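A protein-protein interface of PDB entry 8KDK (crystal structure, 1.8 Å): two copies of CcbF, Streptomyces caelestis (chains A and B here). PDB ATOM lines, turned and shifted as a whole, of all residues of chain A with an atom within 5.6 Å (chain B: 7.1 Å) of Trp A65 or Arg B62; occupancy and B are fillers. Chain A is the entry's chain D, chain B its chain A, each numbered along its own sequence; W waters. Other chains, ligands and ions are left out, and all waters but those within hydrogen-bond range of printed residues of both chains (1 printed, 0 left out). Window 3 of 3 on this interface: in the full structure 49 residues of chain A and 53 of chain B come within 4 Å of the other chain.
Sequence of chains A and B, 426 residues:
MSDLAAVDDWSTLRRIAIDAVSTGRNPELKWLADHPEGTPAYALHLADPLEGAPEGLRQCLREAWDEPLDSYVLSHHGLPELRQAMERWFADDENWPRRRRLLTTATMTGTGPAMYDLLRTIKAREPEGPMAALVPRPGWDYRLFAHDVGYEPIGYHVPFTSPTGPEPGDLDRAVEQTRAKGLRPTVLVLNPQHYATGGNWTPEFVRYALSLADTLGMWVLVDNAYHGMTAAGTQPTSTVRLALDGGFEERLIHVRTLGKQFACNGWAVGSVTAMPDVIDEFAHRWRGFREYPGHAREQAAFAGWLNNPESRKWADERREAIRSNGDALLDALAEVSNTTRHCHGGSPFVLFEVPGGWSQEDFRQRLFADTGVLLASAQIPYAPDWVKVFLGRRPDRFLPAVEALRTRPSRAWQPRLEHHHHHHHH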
ATOM      1  N   LEU A  61       6.556  29.970  19.316  1.00  0.00           N
ATOM      2  CA  LEU A  61       7.676  30.464  20.104  1.00  0.00           C
ATOM      3  C   LEU A  61       8.578  29.323  20.546  1.00  0.00           C
ATOM      4  O   LEU A  61       9.802  29.420  20.452  1.00  0.00           O
ATOM      5  CB  LEU A  61       7.157  31.235  21.316  1.00  0.00           C
ATOM      6  CG  LEU A  61       8.211  31.983  22.122  1.00  0.00           C
ATOM      7  CD1 LEU A  61       8.479  33.328  21.480  1.00  0.00           C
ATOM      8  CD2 LEU A  61       7.679  32.179  23.511  1.00  0.00           C
ATOM      9  N   ARG A  62       7.984  28.243  21.054  1.00  0.00           N
ATOM     10  CA  ARG A  62       8.770  27.110  21.545  1.00  0.00           C
ATOM     11  C   ARG A  62       9.650  26.516  20.449  1.00  0.00           C
ATOM     12  O   ARG A  62      10.839  26.257  20.665  1.00  0.00           O
ATOM     13  CB  ARG A  62       7.830  26.039  22.098  1.00  0.00           C
ATOM     14  CG  ARG A  62       8.528  24.785  22.607  1.00  0.00           C
ATOM     15  CD  ARG A  62       7.512  23.686  22.802  1.00  0.00           C
ATOM     16  NE  ARG A  62       7.163  23.050  21.538  1.00  0.00           N
ATOM     17  CZ  ARG A  62       5.925  22.792  21.143  1.00  0.00           C
ATOM     18  NH1 ARG A  62       4.877  23.158  21.868  1.00  0.00           N
ATOM     19  NH2 ARG A  62       5.733  22.153  19.992  1.00  0.00           N
ATOM     20  N   GLU A  63       9.073  26.253  19.277  1.00  0.00           N
ATOM     21  CA  GLU A  63       9.767  25.513  18.223  1.00  0.00           C
ATOM     22  C   GLU A  63      10.911  26.299  17.599  1.00  0.00           C
ATOM     23  O   GLU A  63      11.766  25.695  16.943  1.00  0.00           O
ATOM     24  CB  GLU A  63       8.760  25.070  17.148  1.00  0.00           C
ATOM     25  CG  GLU A  63       7.920  23.791  17.502  1.00  0.00           C
ATOM     26  CD  GLU A  63       8.744  22.607  18.071  1.00  0.00           C
ATOM     27  OE1 GLU A  63       9.424  21.930  17.275  1.00  0.00           O
ATOM     28  OE2 GLU A  63       8.696  22.316  19.294  1.00  0.00           O
ATOM     29  N   ALA A  64      10.982  27.608  17.823  1.00  0.00           N
ATOM     30  CA  ALA A  64      12.059  28.441  17.306  1.00  0.00           C
ATOM     31  C   ALA A  64      13.144  28.708  18.347  1.00  0.00           C
ATOM     32  O   ALA A  64      14.033  29.523  18.098  1.00  0.00           O
ATOM     33  CB  ALA A  64      11.495  29.771  16.802  1.00  0.00           C
ATOM     34  N   TRP A  65      13.087  28.043  19.501  1.00  0.00           N
ATOM     35  CA  TRP A  65      14.037  28.314  20.579  1.00  0.00           C
ATOM     36  C   TRP A  65      15.493  28.152  20.145  1.00  0.00           C
ATOM     37  O   TRP A  65      16.386  28.743  20.762  1.00  0.00           O
ATOM     38  CB  TRP A  65      13.758  27.384  21.759  1.00  0.00           C
ATOM     39  CG  TRP A  65      14.300  26.010  21.517  1.00  0.00           C
ATOM     40  CD1 TRP A  65      13.684  24.984  20.842  1.00  0.00           C
ATOM     41  CD2 TRP A  65      15.579  25.510  21.930  1.00  0.00           C
ATOM     42  NE1 TRP A  65      14.513  23.881  20.813  1.00  0.00           N
ATOM     43  CE2 TRP A  65      15.678  24.183  21.474  1.00  0.00           C
ATOM     44  CE3 TRP A  65      16.647  26.057  22.650  1.00  0.00           C
ATOM     45  CZ2 TRP A  65      16.803  23.397  21.710  1.00  0.00           C
ATOM     46  CZ3 TRP A  65      17.762  25.270  22.878  1.00  0.00           C
ATOM     47  CH2 TRP A  65      17.830  23.959  22.403  1.00  0.00           C
ATOM     48  N   ASP A  66      15.756  27.368  19.101  1.00  0.00           N
ATOM     49  CA  ASP A  66      17.115  27.083  18.667  1.00  0.00           C
ATOM     50  C   ASP A  66      17.547  27.939  17.489  1.00  0.00           C
ATOM     51  O   ASP A  66      18.630  27.711  16.934  1.00  0.00           O
ATOM     52  CB  ASP A  66      17.248  25.603  18.301  1.00  0.00           C
ATOM     53  CG  ASP A  66      18.420  24.948  18.979  1.00  0.00           C
ATOM     54  OD1 ASP A  66      19.256  25.689  19.546  1.00  0.00           O
ATOM     55  OD2 ASP A  66      18.519  23.699  18.931  1.00  0.00           O
ATOM     56  N   GLU A  67      16.705  28.956  17.082  1.00  0.00           N
ATOM     57  CA  GLU A  67      17.030  29.825  15.967  1.00  0.00           C
ATOM     58  C   GLU A  67      17.664  31.130  16.462  1.00  0.00           C
ATOM     59  O   GLU A  67      17.390  31.575  17.575  1.00  0.00           O
ATOM     60  CB  GLU A  67      15.767  30.124  15.156  1.00  0.00           C
ATOM     61  CG  GLU A  67      15.090  28.839  14.645  1.00  0.00           C
ATOM     62  CD  GLU A  67      13.763  29.102  13.966  1.00  0.00           C
ATOM     63  OE1 GLU A  67      13.539  30.256  13.532  1.00  0.00           O
ATOM     64  OE2 GLU A  67      12.941  28.161  13.871  1.00  0.00           O
ATOM     65  N   ARG A 297      11.823  37.149  18.401  1.00  0.00           N
ATOM     66  CA  ARG A 297      11.163  35.888  18.735  1.00  0.00           C
ATOM     67  C   ARG A 297       9.649  36.050  18.713  1.00  0.00           C
ATOM     68  O   ARG A 297       8.945  35.198  18.162  1.00  0.00           O
ATOM     69  CB  ARG A 297      11.631  35.353  20.091  1.00  0.00           C
ATOM     70  CG  ARG A 297      13.090  34.899  20.075  1.00  0.00           C
ATOM     71  CD  ARG A 297      13.497  34.057  21.300  1.00  0.00           C
ATOM     72  NE  ARG A 297      14.877  33.597  21.146  1.00  0.00           N
ATOM     73  CZ  ARG A 297      15.233  32.579  20.375  1.00  0.00           C
ATOM     74  NH1 ARG A 297      14.328  31.821  19.767  1.00  0.00           N
ATOM     75  NH2 ARG A 297      16.527  32.331  20.185  1.00  0.00           N
ATOM     76  N   ALA B  53      21.563  33.702  21.722  1.00  0.00           N
ATOM     77  CA  ALA B  53      21.811  33.894  23.150  1.00  0.00           C
ATOM     78  C   ALA B  53      22.332  32.591  23.767  1.00  0.00           C
ATOM     79  O   ALA B  53      22.231  31.532  23.142  1.00  0.00           O
ATOM     80  CB  ALA B  53      20.516  34.355  23.836  1.00  0.00           C
ATOM     81  N   PRO B  54      22.918  32.649  24.974  1.00  0.00           N
ATOM     82  CA  PRO B  54      23.450  31.428  25.597  1.00  0.00           C
ATOM     83  C   PRO B  54      22.384  30.358  25.678  1.00  0.00           C
ATOM     84  O   PRO B  54      21.209  30.639  25.937  1.00  0.00           O
ATOM     85  CB  PRO B  54      23.883  31.880  26.997  1.00  0.00           C
ATOM     86  CG  PRO B  54      23.511  33.313  27.118  1.00  0.00           C
ATOM     87  CD  PRO B  54      23.305  33.845  25.740  1.00  0.00           C
ATOM     88  N   GLU B  55      22.815  29.116  25.457  1.00  0.00           N
ATOM     89  CA  GLU B  55      21.862  28.027  25.334  1.00  0.00           C
ATOM     90  C   GLU B  55      21.009  27.891  26.580  1.00  0.00           C
ATOM     91  O   GLU B  55      19.810  27.601  26.486  1.00  0.00           O
ATOM     92  CB  GLU B  55      22.603  26.723  25.065  1.00  0.00           C
ATOM     93  CG  GLU B  55      21.686  25.553  24.947  1.00  0.00           C
ATOM     94  CD  GLU B  55      22.417  24.350  24.443  1.00  0.00           C
ATOM     95  OE1 GLU B  55      23.242  23.817  25.211  1.00  0.00           O
ATOM     96  OE2 GLU B  55      22.184  23.966  23.279  1.00  0.00           O
ATOM     97  N   GLY B  56      21.618  28.063  27.758  1.00  0.00           N
ATOM     98  CA  GLY B  56      20.866  27.932  28.998  1.00  0.00           C
ATOM     99  C   GLY B  56      19.724  28.926  29.089  1.00  0.00           C
ATOM    100  O   GLY B  56      18.656  28.613  29.625  1.00  0.00           O
ATOM    101  N   LEU B  57      19.930  30.137  28.548  1.00  0.00           N
ATOM    102  CA  LEU B  57      18.879  31.153  28.562  1.00  0.00           C
ATOM    103  C   LEU B  57      17.738  30.774  27.626  1.00  0.00           C
ATOM    104  O   LEU B  57      16.561  30.846  27.998  1.00  0.00           O
ATOM    105  CB  LEU B  57      19.474  32.519  28.178  1.00  0.00           C
ATOM    106  CG  LEU B  57      18.492  33.685  28.117  1.00  0.00           C
ATOM    107  CD1 LEU B  57      17.873  33.954  29.497  1.00  0.00           C
ATOM    108  CD2 LEU B  57      19.189  34.920  27.560  1.00  0.00           C
ATOM    109  N   ARG B  58      18.066  30.357  26.403  1.00  0.00           N
ATOM    110  CA  ARG B  58      17.025  29.924  25.472  1.00  0.00           C
ATOM    111  C   ARG B  58      16.305  28.669  25.964  1.00  0.00           C
ATOM    112  O   ARG B  58      15.104  28.499  25.711  1.00  0.00           O
ATOM    113  CB  ARG B  58      17.636  29.698  24.089  1.00  0.00           C
ATOM    114  CG  ARG B  58      18.240  30.971  23.513  1.00  0.00           C
ATOM    115  CD  ARG B  58      18.815  30.759  22.116  1.00  0.00           C
ATOM    116  NE  ARG B  58      20.083  30.033  22.172  1.00  0.00           N
ATOM    117  CZ  ARG B  58      20.239  28.747  21.872  1.00  0.00           C
ATOM    118  NH1 ARG B  58      19.210  27.977  21.523  1.00  0.00           N
ATOM    119  NH2 ARG B  58      21.464  28.220  21.897  1.00  0.00           N
ATOM    120  N   GLN B  59      17.011  27.779  26.664  1.00  0.00           N
ATOM    121  CA  GLN B  59      16.349  26.609  27.238  1.00  0.00           C
ATOM    122  C   GLN B  59      15.309  27.017  28.271  1.00  0.00           C
ATOM    123  O   GLN B  59      14.242  26.401  28.368  1.00  0.00           O
ATOM    124  CB  GLN B  59      17.372  25.681  27.888  1.00  0.00           C
ATOM    125  CG  GLN B  59      18.175  24.898  26.889  1.00  0.00           C
ATOM    126  CD  GLN B  59      19.247  24.033  27.545  1.00  0.00           C
ATOM    127  OE1 GLN B  59      19.861  24.423  28.551  1.00  0.00           O
ATOM    128  NE2 GLN B  59      19.505  22.872  26.949  1.00  0.00           N
ATOM    129  N   CYS B  60      15.630  28.022  29.088  1.00  0.00           N
ATOM    130  CA  CYS B  60      14.680  28.525  30.077  1.00  0.00           C
ATOM    131  C   CYS B  60      13.425  29.065  29.403  1.00  0.00           C
ATOM    132  O   CYS B  60      12.300  28.813  29.856  1.00  0.00           O
ATOM    133  CB  CYS B  60      15.349  29.615  30.915  1.00  0.00           C
ATOM    134  SG  CYS B  60      16.477  29.013  32.181  1.00  0.00           S
ATOM    135  N   LEU B  61      13.606  29.804  28.314  1.00  0.00           N
ATOM    136  CA  LEU B  61      12.476  30.287  27.527  1.00  0.00           C
ATOM    137  C   LEU B  61      11.658  29.135  26.953  1.00  0.00           C
ATOM    138  O   LEU B  61      10.422  29.143  27.011  1.00  0.00           O
ATOM    139  CB  LEU B  61      12.988  31.200  26.418  1.00  0.00           C
ATOM    140  CG  LEU B  61      11.896  31.828  25.547  1.00  0.00           C
ATOM    141  CD1 LEU B  61      11.312  33.041  26.300  1.00  0.00           C
ATOM    142  CD2 LEU B  61      12.458  32.247  24.201  1.00  0.00           C
ATOM    143  N   ARG B  62      12.333  28.130  26.391  1.00  0.00           N
ATOM    144  CA  ARG B  62      11.630  27.037  25.719  1.00  0.00           C
ATOM    145  C   ARG B  62      10.837  26.201  26.707  1.00  0.00           C
ATOM    146  O   ARG B  62       9.705  25.789  26.415  1.00  0.00           O
ATOM    147  CB  ARG B  62      12.638  26.155  24.969  1.00  0.00           C
ATOM    148  CG  ARG B  62      12.081  24.823  24.483  1.00  0.00           C
ATOM    149  CD  ARG B  62      13.212  23.880  24.110  1.00  0.00           C
ATOM    150  NE  ARG B  62      13.698  23.126  25.261  1.00  0.00           N
ATOM    151  CZ  ARG B  62      14.979  22.862  25.499  1.00  0.00           C
ATOM    152  NH1 ARG B  62      15.934  23.284  24.687  1.00  0.00           N
ATOM    153  NH2 ARG B  62      15.310  22.169  26.588  1.00  0.00           N
ATOM    154  N   GLU B  63      11.422  25.933  27.874  1.00  0.00           N
ATOM    155  CA  GLU B  63      10.812  25.028  28.836  1.00  0.00           C
ATOM    156  C   GLU B  63       9.593  25.646  29.493  1.00  0.00           C
ATOM    157  O   GLU B  63       8.765  24.914  30.041  1.00  0.00           O
ATOM    158  CB  GLU B  63      11.839  24.634  29.902  1.00  0.00           C
ATOM    159  CG  GLU B  63      12.912  23.665  29.421  1.00  0.00           C
ATOM    160  CD  GLU B  63      12.334  22.447  28.718  1.00  0.00           C
ATOM    161  OE1 GLU B  63      11.567  21.706  29.363  1.00  0.00           O
ATOM    162  OE2 GLU B  63      12.632  22.237  27.522  1.00  0.00           O
ATOM    163  N   ALA B  64       9.445  26.967  29.429  1.00  0.00           N
ATOM    164  CA  ALA B  64       8.292  27.617  30.048  1.00  0.00           C
ATOM    165  C   ALA B  64       7.176  27.909  29.047  1.00  0.00           C
ATOM    166  O   ALA B  64       6.227  28.618  29.386  1.00  0.00           O
ATOM    167  CB  ALA B  64       8.732  28.899  30.764  1.00  0.00           C
ATOM    168  N   TRP B  65       7.236  27.318  27.850  1.00  0.00           N
ATOM    169  CA  TRP B  65       6.271  27.631  26.800  1.00  0.00           C
ATOM    170  C   TRP B  65       4.849  27.321  27.217  1.00  0.00           C
ATOM    171  O   TRP B  65       3.913  27.921  26.689  1.00  0.00           O
ATOM    172  CB  TRP B  65       6.591  26.858  25.516  1.00  0.00           C
ATOM    173  CG  TRP B  65       6.221  25.416  25.624  1.00  0.00           C
ATOM    174  CD1 TRP B  65       6.977  24.417  26.181  1.00  0.00           C
ATOM    175  CD2 TRP B  65       4.983  24.803  25.217  1.00  0.00           C
ATOM    176  NE1 TRP B  65       6.295  23.230  26.128  1.00  0.00           N
ATOM    177  CE2 TRP B  65       5.067  23.439  25.553  1.00  0.00           C
ATOM    178  CE3 TRP B  65       3.822  25.275  24.594  1.00  0.00           C
ATOM    179  CZ2 TRP B  65       4.041  22.530  25.271  1.00  0.00           C
ATOM    180  CZ3 TRP B  65       2.793  24.371  24.330  1.00  0.00           C
ATOM    181  CH2 TRP B  65       2.915  23.018  24.672  1.00  0.00           C
ATOM    182  N   ASP B  66       4.655  26.391  28.148  1.00  0.00           N
ATOM    183  CA  ASP B  66       3.310  26.001  28.536  1.00  0.00           C
ATOM    184  C   ASP B  66       2.915  26.620  29.872  1.00  0.00           C
ATOM    185  O   ASP B  66       1.905  26.223  30.453  1.00  0.00           O
ATOM    186  CB  ASP B  66       3.192  24.472  28.597  1.00  0.00           C
ATOM    187  CG  ASP B  66       1.758  23.981  28.436  1.00  0.00           C
ATOM    188  OD1 ASP B  66       0.926  24.705  27.838  1.00  0.00           O
ATOM    189  OD2 ASP B  66       1.477  22.826  28.821  1.00  0.00           O
ATOM    190  N   ARG B 297       7.726  36.568  29.636  1.00  0.00           N
ATOM    191  CA  ARG B 297       8.475  35.414  29.145  1.00  0.00           C
ATOM    192  C   ARG B 297       9.978  35.679  29.183  1.00  0.00           C
ATOM    193  O   ARG B 297      10.750  34.871  29.722  1.00  0.00           O
ATOM    194  CB  ARG B 297       7.998  35.064  27.736  1.00  0.00           C
ATOM    195  CG  ARG B 297       6.665  34.363  27.790  1.00  0.00           C
ATOM    196  CD  ARG B 297       6.373  33.524  26.580  1.00  0.00           C
ATOM    197  NE  ARG B 297       5.054  32.920  26.730  1.00  0.00           N
ATOM    198  CZ  ARG B 297       4.820  31.793  27.385  1.00  0.00           C
ATOM    199  NH1 ARG B 297       5.803  31.094  27.946  1.00  0.00           N
ATOM    200  NH2 ARG B 297       3.565  31.368  27.511  1.00  0.00           N
ATOM    201  N   ALA B 301      12.499  33.831  31.907  1.00  0.00           N
ATOM    202  CA  ALA B 301      13.646  33.106  31.367  1.00  0.00           C
ATOM    203  C   ALA B 301      14.941  33.636  31.964  1.00  0.00           C
ATOM    204  O   ALA B 301      15.813  32.856  32.356  1.00  0.00           O
ATOM    205  CB  ALA B 301      13.666  33.198  29.836  1.00  0.00           C
HETATM  206  O   HOH W   1      21.413  25.327  20.873  1.00  0.00           O
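OD1 of Asp A66 is in salt-bridge range of NH1 of Arg B58 (3.0 Å). The guanidinium group (NH1) of Arg B58 is in hydrogen-bond range of the backbone carbonyl oxygen (O) of Trp A65, 3.0 Å away.
The side-chain carboxylate (OE2) of Glu A63 lies within salt-bridge range of the guanidinium group (NE) of Arg A62 (2.8 Å). O of Ala A64 is in hydrogen-bond range of NH1 of Arg A297, 2.9 Å away. NE of Arg B62 lies within salt-bridge range of OE2 of Glu B63 (2.7 Å). NE of Arg B58 sits at hydrogen-bond distance from O of Ala B53 (2.8 Å). The guanidinium group (NH2) of Arg A297 is in hydrogen-bond range of the backbone carbonyl oxygen (O) of Glu A67 (2.9 Å). NH1 of Arg B297 is in hydrogen-bond range of O of Ala B64, at 2.9 Å.
Leu A61 touches Arg B297 (CD2 to CD, 3.6 Å). Trp B65 touches Arg A62. Trp A65 touches Arg B62. NH2 of Arg A297 touches CD of Arg B58 (3.4 Å). Arg A297 touches Leu B61.
Of the printed residues of chain B, Arg A62 touches Trp B65 (3.4 Å). Of chain B, only Arg B58 (3.0 Å) and Arg B62 (3.0 Å) come within 4 Å of Trp A65. Of the printed residues of chain B, Arg A297 touches Arg B58 (3.4 Å) and Leu B61 (3.6 Å). Ala B53 touches none of the printed residues of chain A. Pro B54 touches none of the printed residues of chain A. Of the printed residues of chain A, Arg B58 touches Trp A65 (3.0 Å), Asp A66 (3.0 Å) and Arg A297 (3.4 Å). Printed residues of chain A within 4 Å of Arg B62: Trp A65. Printed residues of chain A within 4 Å of Trp B65: Arg A62. Of the printed residues of chain A, Arg B297 touches Leu A61 (3.6 Å). The nearest printed residue of chain A that does not touch Arg B62 is Arg A62 (4.02 Å). The nearest printed residue of chain B that does not touch Leu A61 is Leu B61 (4.7 Å).
Of the 16 printed residues of chain B, 5 touch a printed residue of chain A. Among the printed residues, 7 pairs touch across the chains. Among the printed residues, Asp or Glu carboxylates within 4 Å of a Lys or Arg side-chain nitrogen of the other chain: Asp A66 with Arg B58 (3.0 Å).
Leu A61 touches Arg B297, and with the chains exchanged Arg A297 touches Leu B61. Arg A62 touches Trp B65, and with the chains exchanged Trp A65 touches Arg B62. Positions printed for both chains: 61, 62, 63, 64, 65, 66 and 297. Of the 7 pairs that touch across the chains among the printed residues, 4 have their exchanged pair printed and touching as well.
Water W1 lies within hydrogen-bond range of the side-chain carboxylate (OD1) of Asp A66, the side-chain carboxylate (OE2) of Glu B55 and the guanidinium group (NH2) of Arg B58.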
